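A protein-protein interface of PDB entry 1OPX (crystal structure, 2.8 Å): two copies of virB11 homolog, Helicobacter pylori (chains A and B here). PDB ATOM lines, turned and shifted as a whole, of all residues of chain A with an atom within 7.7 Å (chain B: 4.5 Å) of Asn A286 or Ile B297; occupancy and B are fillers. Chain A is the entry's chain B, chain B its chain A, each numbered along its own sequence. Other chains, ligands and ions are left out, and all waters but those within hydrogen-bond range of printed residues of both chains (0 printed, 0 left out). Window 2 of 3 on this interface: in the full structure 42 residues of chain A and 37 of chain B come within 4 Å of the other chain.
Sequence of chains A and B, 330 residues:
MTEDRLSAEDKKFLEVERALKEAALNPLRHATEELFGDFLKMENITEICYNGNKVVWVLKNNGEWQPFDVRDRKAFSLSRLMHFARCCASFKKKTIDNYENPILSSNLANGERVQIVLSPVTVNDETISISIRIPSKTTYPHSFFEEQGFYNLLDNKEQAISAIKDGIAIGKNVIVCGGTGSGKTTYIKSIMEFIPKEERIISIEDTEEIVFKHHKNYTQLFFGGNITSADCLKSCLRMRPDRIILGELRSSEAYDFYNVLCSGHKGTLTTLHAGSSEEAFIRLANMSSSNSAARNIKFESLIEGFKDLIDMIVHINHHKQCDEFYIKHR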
ATOM      1  N   ARG A 250      -4.445   7.864  -0.484  1.00  0.00           N
ATOM      2  CA  ARG A 250      -5.107   6.571  -0.707  1.00  0.00           C
ATOM      3  C   ARG A 250      -5.978   6.531  -1.971  1.00  0.00           C
ATOM      4  O   ARG A 250      -5.671   5.795  -2.911  1.00  0.00           O
ATOM      5  CB  ARG A 250      -5.937   6.168   0.522  1.00  0.00           C
ATOM      6  CG  ARG A 250      -7.075   5.194   0.202  1.00  0.00           C
ATOM      7  CD  ARG A 250      -7.485   4.297   1.382  1.00  0.00           C
ATOM      8  NE  ARG A 250      -7.195   4.888   2.687  1.00  0.00           N
ATOM      9  CZ  ARG A 250      -7.484   4.312   3.852  1.00  0.00           C
ATOM     10  NH1 ARG A 250      -8.084   3.126   3.892  1.00  0.00           N
ATOM     11  NH2 ARG A 250      -7.153   4.913   4.986  1.00  0.00           N
ATOM     12  N   SER A 251      -7.063   7.304  -1.988  1.00  0.00           N
ATOM     13  CA  SER A 251      -7.955   7.358  -3.145  1.00  0.00           C
ATOM     14  C   SER A 251      -9.077   8.350  -2.900  1.00  0.00           C
ATOM     15  O   SER A 251      -9.562   8.981  -3.836  1.00  0.00           O
ATOM     16  CB  SER A 251      -8.553   5.981  -3.448  1.00  0.00           C
ATOM     17  OG  SER A 251      -9.415   5.563  -2.414  1.00  0.00           O
ATOM     18  N   ALA A 254      -7.420  11.587  -2.958  1.00  0.00           N
ATOM     19  CA  ALA A 254      -6.855  11.603  -4.299  1.00  0.00           C
ATOM     20  C   ALA A 254      -7.258  12.830  -5.122  1.00  0.00           C
ATOM     21  O   ALA A 254      -6.407  13.680  -5.418  1.00  0.00           O
ATOM     22  CB  ALA A 254      -7.231  10.339  -5.023  1.00  0.00           C
ATOM     23  N   GLU A 279       5.443   7.041 -12.760  1.00  0.00           N
ATOM     24  CA  GLU A 279       4.387   6.243 -12.175  1.00  0.00           C
ATOM     25  C   GLU A 279       3.546   7.071 -11.215  1.00  0.00           C
ATOM     26  O   GLU A 279       2.317   7.048 -11.275  1.00  0.00           O
ATOM     27  CB  GLU A 279       4.980   5.053 -11.431  1.00  0.00           C
ATOM     28  CG  GLU A 279       4.867   3.728 -12.172  1.00  0.00           C
ATOM     29  CD  GLU A 279       5.623   2.621 -11.474  1.00  0.00           C
ATOM     30  OE1 GLU A 279       5.396   2.438 -10.259  1.00  0.00           O
ATOM     31  OE2 GLU A 279       6.440   1.943 -12.139  1.00  0.00           O
ATOM     32  N   ALA A 280       4.210   7.790 -10.319  1.00  0.00           N
ATOM     33  CA  ALA A 280       3.496   8.613  -9.360  1.00  0.00           C
ATOM     34  C   ALA A 280       2.412   9.486 -10.000  1.00  0.00           C
ATOM     35  O   ALA A 280       1.331   9.645  -9.421  1.00  0.00           O
ATOM     36  CB  ALA A 280       4.470   9.481  -8.594  1.00  0.00           C
ATOM     37  N   PHE A 281       2.678  10.047 -11.184  1.00  0.00           N
ATOM     38  CA  PHE A 281       1.676  10.906 -11.826  1.00  0.00           C
ATOM     39  C   PHE A 281       0.411  10.140 -12.254  1.00  0.00           C
ATOM     40  O   PHE A 281      -0.714  10.628 -12.109  1.00  0.00           O
ATOM     41  CB  PHE A 281       2.294  11.645 -13.024  1.00  0.00           C
ATOM     42  CG  PHE A 281       3.298  12.715 -12.636  1.00  0.00           C
ATOM     43  CD1 PHE A 281       4.653  12.532 -12.874  1.00  0.00           C
ATOM     44  CD2 PHE A 281       2.881  13.919 -12.062  1.00  0.00           C
ATOM     45  CE1 PHE A 281       5.571  13.525 -12.554  1.00  0.00           C
ATOM     46  CE2 PHE A 281       3.796  14.920 -11.739  1.00  0.00           C
ATOM     47  CZ  PHE A 281       5.135  14.724 -11.986  1.00  0.00           C
ATOM     48  N   ILE A 282       0.614   8.933 -12.767  1.00  0.00           N
ATOM     49  CA  ILE A 282      -0.471   8.063 -13.216  1.00  0.00           C
ATOM     50  C   ILE A 282      -1.221   7.514 -12.000  1.00  0.00           C
ATOM     51  O   ILE A 282      -2.448   7.377 -12.000  1.00  0.00           O
ATOM     52  CB  ILE A 282       0.105   6.892 -14.031  1.00  0.00           C
ATOM     53  CG1 ILE A 282       0.776   7.438 -15.283  1.00  0.00           C
ATOM     54  CG2 ILE A 282      -0.988   5.921 -14.419  1.00  0.00           C
ATOM     55  CD1 ILE A 282       1.608   6.429 -16.010  1.00  0.00           C
ATOM     56  N   ARG A 283      -0.456   7.184 -10.971  1.00  0.00           N
ATOM     57  CA  ARG A 283      -1.003   6.681  -9.730  1.00  0.00           C
ATOM     58  C   ARG A 283      -2.028   7.727  -9.274  1.00  0.00           C
ATOM     59  O   ARG A 283      -3.155   7.397  -8.898  1.00  0.00           O
ATOM     60  CB  ARG A 283       0.132   6.576  -8.716  1.00  0.00           C
ATOM     61  CG  ARG A 283      -0.042   5.516  -7.669  1.00  0.00           C
ATOM     62  CD  ARG A 283      -0.065   4.147  -8.302  1.00  0.00           C
ATOM     63  NE  ARG A 283      -1.403   3.578  -8.228  1.00  0.00           N
ATOM     64  CZ  ARG A 283      -2.029   3.304  -7.086  1.00  0.00           C
ATOM     65  NH1 ARG A 283      -1.433   3.543  -5.918  1.00  0.00           N
ATOM     66  NH2 ARG A 283      -3.262   2.808  -7.113  1.00  0.00           N
ATOM     67  N   LEU A 284      -1.622   8.996  -9.337  1.00  0.00           N
ATOM     68  CA  LEU A 284      -2.453  10.131  -8.939  1.00  0.00           C
ATOM     69  C   LEU A 284      -3.712  10.274  -9.785  1.00  0.00           C
ATOM     70  O   LEU A 284      -4.812  10.384  -9.254  1.00  0.00           O
ATOM     71  CB  LEU A 284      -1.621  11.410  -9.008  1.00  0.00           C
ATOM     72  CG  LEU A 284      -0.467  11.431  -8.008  1.00  0.00           C
ATOM     73  CD1 LEU A 284       0.444  12.614  -8.271  1.00  0.00           C
ATOM     74  CD2 LEU A 284      -1.041  11.468  -6.593  1.00  0.00           C
ATOM     75  N   ALA A 285      -3.537  10.283 -11.104  1.00  0.00           N
ATOM     76  CA  ALA A 285      -4.649  10.374 -12.047  1.00  0.00           C
ATOM     77  C   ALA A 285      -5.636   9.243 -11.775  1.00  0.00           C
ATOM     78  O   ALA A 285      -6.814   9.493 -11.537  1.00  0.00           O
ATOM     79  CB  ALA A 285      -4.129  10.277 -13.455  1.00  0.00           C
ATOM     80  N   ASN A 286      -5.154   8.001 -11.808  1.00  0.00           N
ATOM     81  CA  ASN A 286      -6.002   6.838 -11.539  1.00  0.00           C
ATOM     82  C   ASN A 286      -6.891   7.088 -10.338  1.00  0.00           C
ATOM     83  O   ASN A 286      -8.120   6.981 -10.412  1.00  0.00           O
ATOM     84  CB  ASN A 286      -5.154   5.612 -11.211  1.00  0.00           C
ATOM     85  CG  ASN A 286      -4.406   5.086 -12.394  1.00  0.00           C
ATOM     86  OD1 ASN A 286      -3.607   4.151 -12.271  1.00  0.00           O
ATOM     87  ND2 ASN A 286      -4.657   5.672 -13.556  1.00  0.00           N
ATOM     88  N   MET A 287      -6.235   7.400  -9.222  1.00  0.00           N
ATOM     89  CA  MET A 287      -6.904   7.653  -7.956  1.00  0.00           C
ATOM     90  C   MET A 287      -7.909   8.790  -8.041  1.00  0.00           C
ATOM     91  O   MET A 287      -9.066   8.625  -7.669  1.00  0.00           O
ATOM     92  CB  MET A 287      -5.872   7.950  -6.855  1.00  0.00           C
ATOM     93  CG  MET A 287      -5.014   6.748  -6.428  1.00  0.00           C
ATOM     94  SD  MET A 287      -3.804   7.106  -4.932  1.00  0.00           S
ATOM     95  CE  MET A 287      -2.493   8.157  -5.877  1.00  0.00           C
ATOM     96  N   SER A 288      -7.479   9.941  -8.530  1.00  0.00           N
ATOM     97  CA  SER A 288      -8.378  11.078  -8.634  1.00  0.00           C
ATOM     98  C   SER A 288      -9.629  10.731  -9.449  1.00  0.00           C
ATOM     99  O   SER A 288     -10.751  11.097  -9.074  1.00  0.00           O
ATOM    100  CB  SER A 288      -7.651  12.256  -9.288  1.00  0.00           C
ATOM    101  OG  SER A 288      -6.402  12.514  -8.664  1.00  0.00           O
ATOM    102  N   SER A 289      -9.419  10.022 -10.558  1.00  0.00           N
ATOM    103  CA  SER A 289     -10.488   9.621 -11.474  1.00  0.00           C
ATOM    104  C   SER A 289     -11.604   8.871 -10.780  1.00  0.00           C
ATOM    105  O   SER A 289     -12.780   9.043 -11.111  1.00  0.00           O
ATOM    106  CB  SER A 289      -9.930   8.730 -12.584  1.00  0.00           C
ATOM    107  OG  SER A 289      -8.840   9.340 -13.242  1.00  0.00           O
ATOM    108  N   SER A 290     -11.230   8.024  -9.830  1.00  0.00           N
ATOM    109  CA  SER A 290     -12.207   7.229  -9.104  1.00  0.00           C
ATOM    110  C   SER A 290     -13.195   8.091  -8.337  1.00  0.00           C
ATOM    111  O   SER A 290     -14.184   7.579  -7.822  1.00  0.00           O
ATOM    112  CB  SER A 290     -11.512   6.260  -8.137  1.00  0.00           C
ATOM    113  OG  SER A 290     -10.834   6.943  -7.098  1.00  0.00           O
ATOM    114  N   ASN A 291     -12.935   9.393  -8.253  1.00  0.00           N
ATOM    115  CA  ASN A 291     -13.851  10.260  -7.533  1.00  0.00           C
ATOM    116  C   ASN A 291     -14.964  10.751  -8.434  1.00  0.00           C
ATOM    117  O   ASN A 291     -14.736  11.130  -9.581  1.00  0.00           O
ATOM    118  CB  ASN A 291     -13.144  11.467  -6.930  1.00  0.00           C
ATOM    119  CG  ASN A 291     -13.963  12.102  -5.825  1.00  0.00           C
ATOM    120  OD1 ASN A 291     -14.101  11.528  -4.741  1.00  0.00           O
ATOM    121  ND2 ASN A 291     -14.538  13.273  -6.097  1.00  0.00           N
ATOM    122  N   ILE A 297     -13.922  14.790 -16.226  1.00  0.00           N
ATOM    123  CA  ILE A 297     -12.634  15.363 -16.600  1.00  0.00           C
ATOM    124  C   ILE A 297     -11.739  14.329 -17.281  1.00  0.00           C
ATOM    125  O   ILE A 297     -11.548  13.216 -16.778  1.00  0.00           O
ATOM    126  CB  ILE A 297     -11.943  15.963 -15.358  1.00  0.00           C
ATOM    127  N   PHE A 299      -9.001  11.913 -18.498  1.00  0.00           N
ATOM    128  CA  PHE A 299      -7.948  11.222 -17.758  1.00  0.00           C
ATOM    129  C   PHE A 299      -6.543  11.792 -17.965  1.00  0.00           C
ATOM    130  O   PHE A 299      -5.794  11.978 -17.005  1.00  0.00           O
ATOM    131  CB  PHE A 299      -7.931   9.741 -18.116  1.00  0.00           C
ATOM    132  CG  PHE A 299      -6.904   8.967 -17.362  1.00  0.00           C
ATOM    133  CD1 PHE A 299      -7.051   8.747 -15.994  1.00  0.00           C
ATOM    134  CD2 PHE A 299      -5.780   8.468 -18.009  1.00  0.00           C
ATOM    135  CE1 PHE A 299      -6.093   8.041 -15.283  1.00  0.00           C
ATOM    136  CE2 PHE A 299      -4.814   7.759 -17.306  1.00  0.00           C
ATOM    137  CZ  PHE A 299      -4.971   7.544 -15.940  1.00  0.00           C
ATOM    138  N   GLU A 300      -6.167  12.042 -19.214  1.00  0.00           N
ATOM    139  CA  GLU A 300      -4.843  12.597 -19.475  1.00  0.00           C
ATOM    140  C   GLU A 300      -4.759  13.998 -18.872  1.00  0.00           C
ATOM    141  O   GLU A 300      -3.675  14.469 -18.522  1.00  0.00           O
ATOM    142  CB  GLU A 300      -4.573  12.651 -20.975  1.00  0.00           C
ATOM    143  N   LEU A 302      -5.831  14.896 -16.015  1.00  0.00           N
ATOM    144  CA  LEU A 302      -5.501  14.798 -14.596  1.00  0.00           C
ATOM    145  C   LEU A 302      -3.998  14.607 -14.489  1.00  0.00           C
ATOM    146  O   LEU A 302      -3.336  15.262 -13.689  1.00  0.00           O
ATOM    147  CB  LEU A 302      -6.210  13.608 -13.942  1.00  0.00           C
ATOM    148  CG  LEU A 302      -7.719  13.742 -13.718  1.00  0.00           C
ATOM    149  CD1 LEU A 302      -8.264  12.500 -13.031  1.00  0.00           C
ATOM    150  CD2 LEU A 302      -7.983  14.978 -12.864  1.00  0.00           C
ATOM    151  N   ILE A 303      -3.461  13.705 -15.302  1.00  0.00           N
ATOM    152  CA  ILE A 303      -2.031  13.454 -15.287  1.00  0.00           C
ATOM    153  C   ILE A 303      -1.295  14.765 -15.503  1.00  0.00           C
ATOM    154  O   ILE A 303      -0.397  15.112 -14.743  1.00  0.00           O
ATOM    155  CB  ILE A 303      -1.608  12.447 -16.380  1.00  0.00           C
ATOM    156  CG1 ILE A 303      -2.193  11.063 -16.061  1.00  0.00           C
ATOM    157  CG2 ILE A 303      -0.091  12.389 -16.467  1.00  0.00           C
ATOM    158  CD1 ILE A 303      -1.213   9.901 -16.210  1.00  0.00           C
ATOM    159  N   PHE A 306      -1.344  17.006 -12.286  1.00  0.00           N
ATOM    160  CA  PHE A 306      -0.342  16.822 -11.252  1.00  0.00           C
ATOM    161  C   PHE A 306       1.045  17.199 -11.756  1.00  0.00           C
ATOM    162  O   PHE A 306       1.888  17.677 -10.992  1.00  0.00           O
ATOM    163  CB  PHE A 306      -0.334  15.367 -10.776  1.00  0.00           C
ATOM    164  CG  PHE A 306      -1.573  14.970 -10.029  1.00  0.00           C
ATOM    165  CD1 PHE A 306      -2.743  14.635 -10.711  1.00  0.00           C
ATOM    166  CD2 PHE A 306      -1.593  15.002  -8.638  1.00  0.00           C
ATOM    167  CE1 PHE A 306      -3.920  14.342 -10.009  1.00  0.00           C
ATOM    168  CE2 PHE A 306      -2.752  14.716  -7.932  1.00  0.00           C
ATOM    169  CZ  PHE A 306      -3.925  14.385  -8.617  1.00  0.00           C
ATOM    170  N   TYR B 255      -8.659  -5.053 -11.718  1.00  0.00           N
ATOM    171  CA  TYR B 255      -8.161  -3.685 -11.583  1.00  0.00           C
ATOM    172  C   TYR B 255      -7.313  -3.461 -10.334  1.00  0.00           C
ATOM    173  O   TYR B 255      -6.328  -2.731 -10.373  1.00  0.00           O
ATOM    174  CB  TYR B 255      -9.321  -2.688 -11.589  1.00  0.00           C
ATOM    175  CG  TYR B 255      -8.839  -1.260 -11.501  1.00  0.00           C
ATOM    176  CD1 TYR B 255      -8.106  -0.699 -12.540  1.00  0.00           C
ATOM    177  CD2 TYR B 255      -9.037  -0.504 -10.340  1.00  0.00           C
ATOM    178  CE1 TYR B 255      -7.575   0.562 -12.431  1.00  0.00           C
ATOM    179  CE2 TYR B 255      -8.511   0.761 -10.217  1.00  0.00           C
ATOM    180  CZ  TYR B 255      -7.773   1.290 -11.267  1.00  0.00           C
ATOM    181  OH  TYR B 255      -7.208   2.540 -11.154  1.00  0.00           O
ATOM    182  N   TYR B 258      -3.951  -4.215 -11.169  1.00  0.00           N
ATOM    183  CA  TYR B 258      -3.313  -3.184 -11.993  1.00  0.00           C
ATOM    184  C   TYR B 258      -2.706  -2.136 -11.068  1.00  0.00           C
ATOM    185  O   TYR B 258      -1.630  -1.600 -11.326  1.00  0.00           O
ATOM    186  CB  TYR B 258      -4.363  -2.517 -12.907  1.00  0.00           C
ATOM    187  CG  TYR B 258      -3.892  -1.240 -13.604  1.00  0.00           C
ATOM    188  CD1 TYR B 258      -2.793  -1.258 -14.462  1.00  0.00           C
ATOM    189  CD2 TYR B 258      -4.543  -0.017 -13.396  1.00  0.00           C
ATOM    190  CE1 TYR B 258      -2.346  -0.098 -15.094  1.00  0.00           C
ATOM    191  CE2 TYR B 258      -4.109   1.149 -14.023  1.00  0.00           C
ATOM    192  CZ  TYR B 258      -3.002   1.102 -14.870  1.00  0.00           C
ATOM    193  OH  TYR B 258      -2.519   2.247 -15.477  1.00  0.00           O
ATOM    194  N   ASN B 259      -3.432  -1.847  -9.993  1.00  0.00           N
ATOM    195  CA  ASN B 259      -2.991  -0.882  -9.007  1.00  0.00           C
ATOM    196  C   ASN B 259      -1.820  -1.411  -8.221  1.00  0.00           C
ATOM    197  O   ASN B 259      -0.831  -0.706  -8.059  1.00  0.00           O
ATOM    198  CB  ASN B 259      -4.119  -0.525  -8.054  1.00  0.00           C
ATOM    199  CG  ASN B 259      -5.076   0.467  -8.654  1.00  0.00           C
ATOM    200  OD1 ASN B 259      -4.661   1.424  -9.318  1.00  0.00           O
ATOM    201  ND2 ASN B 259      -6.365   0.259  -8.420  1.00  0.00           N
ATOM    202  N   CYS B 262       0.952  -0.702 -10.270  1.00  0.00           N
ATOM    203  CA  CYS B 262       1.190   0.735 -10.405  1.00  0.00           C
ATOM    204  C   CYS B 262       2.060   1.244  -9.260  1.00  0.00           C
ATOM    205  O   CYS B 262       2.932   2.084  -9.463  1.00  0.00           O
ATOM    206  CB  CYS B 262      -0.131   1.499 -10.385  1.00  0.00           C
ATOM    207  SG  CYS B 262      -0.989   1.623 -11.975  1.00  0.00           S
ATOM    208  N   ALA B 294     -12.124   2.025 -12.259  1.00  0.00           N
ATOM    209  CA  ALA B 294     -11.494   2.330 -13.546  1.00  0.00           C
ATOM    210  C   ALA B 294     -12.510   2.924 -14.521  1.00  0.00           C
ATOM    211  O   ALA B 294     -12.293   2.945 -15.729  1.00  0.00           O
ATOM    212  CB  ALA B 294     -10.897   1.060 -14.130  1.00  0.00           C
ATOM    213  N   ARG B 295     -13.622   3.409 -13.985  1.00  0.00           N
ATOM    214  CA  ARG B 295     -14.676   3.981 -14.805  1.00  0.00           C
ATOM    215  C   ARG B 295     -14.228   5.221 -15.559  1.00  0.00           C
ATOM    216  O   ARG B 295     -14.776   5.531 -16.610  1.00  0.00           O
ATOM    217  CB  ARG B 295     -15.875   4.313 -13.947  1.00  0.00           C
ATOM    218  N   ASN B 296     -13.232   5.931 -15.037  1.00  0.00           N
ATOM    219  CA  ASN B 296     -12.769   7.150 -15.695  1.00  0.00           C
ATOM    220  C   ASN B 296     -11.373   7.030 -16.312  1.00  0.00           C
ATOM    221  O   ASN B 296     -10.685   8.031 -16.516  1.00  0.00           O
ATOM    222  CB  ASN B 296     -12.815   8.317 -14.703  1.00  0.00           C
ATOM    223  N   ILE B 297     -10.960   5.806 -16.620  1.00  0.00           N
ATOM    224  CA  ILE B 297      -9.646   5.573 -17.209  1.00  0.00           C
ATOM    225  C   ILE B 297      -9.750   5.076 -18.659  1.00  0.00           C
ATOM    226  O   ILE B 297     -10.477   4.123 -18.958  1.00  0.00           O
ATOM    227  CB  ILE B 297      -8.834   4.528 -16.375  1.00  0.00           C
ATOM    228  CG1 ILE B 297      -8.466   5.098 -15.004  1.00  0.00           C
ATOM    229  CG2 ILE B 297      -7.565   4.135 -17.118  1.00  0.00           C
ATOM    230  CD1 ILE B 297      -7.634   4.133 -14.162  1.00  0.00           C
ATOM    231  N   LYS B 298      -9.017   5.727 -19.557  1.00  0.00           N
ATOM    232  CA  LYS B 298      -9.028   5.339 -20.962  1.00  0.00           C
ATOM    233  C   LYS B 298      -8.655   3.854 -21.143  1.00  0.00           C
ATOM    234  O   LYS B 298      -7.656   3.386 -20.599  1.00  0.00           O
ATOM    235  CB  LYS B 298      -8.067   6.236 -21.744  1.00  0.00           C
ATOM    236  N   PHE B 299      -9.459   3.119 -21.908  1.00  0.00           N
ATOM    237  CA  PHE B 299      -9.211   1.698 -22.135  1.00  0.00           C
ATOM    238  C   PHE B 299      -7.815   1.366 -22.665  1.00  0.00           C
ATOM    239  O   PHE B 299      -7.170   0.433 -22.184  1.00  0.00           O
ATOM    240  CB  PHE B 299     -10.236   1.120 -23.097  1.00  0.00           C
ATOM    241  CG  PHE B 299     -10.028  -0.340 -23.374  1.00  0.00           C
ATOM    242  CD1 PHE B 299     -10.397  -1.295 -22.431  1.00  0.00           C
ATOM    243  CD2 PHE B 299      -9.431  -0.761 -24.560  1.00  0.00           C
ATOM    244  CE1 PHE B 299     -10.177  -2.652 -22.663  1.00  0.00           C
ATOM    245  CE2 PHE B 299      -9.206  -2.114 -24.801  1.00  0.00           C
ATOM    246  CZ  PHE B 299      -9.578  -3.062 -23.851  1.00  0.00           C
ATOM    247  N   SER B 301      -5.339   3.038 -22.208  1.00  0.00           N
ATOM    248  CA  SER B 301      -4.460   3.438 -21.110  1.00  0.00           C
ATOM    249  C   SER B 301      -4.221   2.291 -20.136  1.00  0.00           C
ATOM    250  O   SER B 301      -3.199   2.253 -19.458  1.00  0.00           O
ATOM    251  CB  SER B 301      -5.057   4.638 -20.374  1.00  0.00           C
ATOM    252  N   LEU B 302      -5.174   1.364 -20.058  1.00  0.00           N
ATOM    253  CA  LEU B 302      -5.032   0.208 -19.180  1.00  0.00           C
ATOM    254  C   LEU B 302      -4.106  -0.779 -19.873  1.00  0.00           C
ATOM    255  O   LEU B 302      -3.178  -1.302 -19.267  1.00  0.00           O
ATOM    256  CB  LEU B 302      -6.385  -0.450 -18.917  1.00  0.00           C
ATOM    257  CG  LEU B 302      -7.391   0.406 -18.142  1.00  0.00           C
ATOM    258  CD1 LEU B 302      -8.742  -0.302 -18.090  1.00  0.00           C
ATOM    259  CD2 LEU B 302      -6.861   0.668 -16.731  1.00  0.00           C
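NH2 of Arg A283 is in hydrogen-bond range of OD1 of Asn B259 (3.0 Å). OD1 of Asn A286 is in hydrogen-bond range of SG of Cys B262. The backbone carbonyl oxygen (O) of Cys B262 sits close to the side-chain carboxylate (OE1) of Glu A279 (2.6 Å).
The side-chain sulfur (SG) of Cys B262 lies within hydrogen-bond range of the backbone carbonyl oxygen (O) of Tyr B258 (3.3 Å). The side-chain hydroxyl (OG) of Ser A289 is in hydrogen-bond range of the backbone carbonyl oxygen (O) of Ala A285, at 2.7 Å. O of Ile A282 sits close to ND2 of Asn A286 (3.2 Å). The side-chain amide oxygen of Asn B259 sits at hydrogen-bond distance from the side-chain hydroxyl of Tyr B255, at 3.3 Å.
Among the printed residues, pairs that only touch across the chains: Arg A283 with Cys B262 (3.3 Å), Asn A286 with Tyr B255 (3.7 Å), Asn A286 with Tyr B258 (3.5 Å), Asn A286 with Ile B297 (3.4 Å), Ser A289 with Asn B296 (3.6 Å), Phe A299 with Asn B296 (3.6 Å) and Phe A299 with Ile B297 (3.8 Å).
Of chain B, only Tyr B255, Tyr B258, Cys B262 and Ile B297 come within 4 Å of Asn A286. Of chain A, only Asn A286 (3.4 Å) and Phe A299 (3.8 Å) come within 4 Å of Ile B297. Printed residues of chain B within 4 Å of Arg A283: Asn B259 (3.0 Å) and Cys B262 (3.3 Å). Of the printed residues of chain A, Tyr B258 touches Asn A286. Leu A302 touches none of the printed residues of chain B. The nearest residue of chain B that does not touch Asn A286 is Asn B259 (4.2 Å). The nearest residue of chain A that does not touch Ile B297 is Ser A289 (4.6 Å). The nearest printed residue of chain B that does not touch Arg A283 is Tyr B255 (5.7 Å).
Hydrophobic or aromatic side chains of chain A within 4 Å of the printed part of chain B: Phe A299. Along chain A the printed residues that touch a printed residue of chain B span positions 279 to 299. Among the printed residues, 10 pairs touch across the chains.
Phe A299 touches Ile B297, but with the chains exchanged Ile A297 does not touch Phe B299 (11.5 Å). 3 positions are printed for both chains. Of the 10 pairs that touch across the chains among the printed residues, none has its exchanged pair printed and touching as well.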
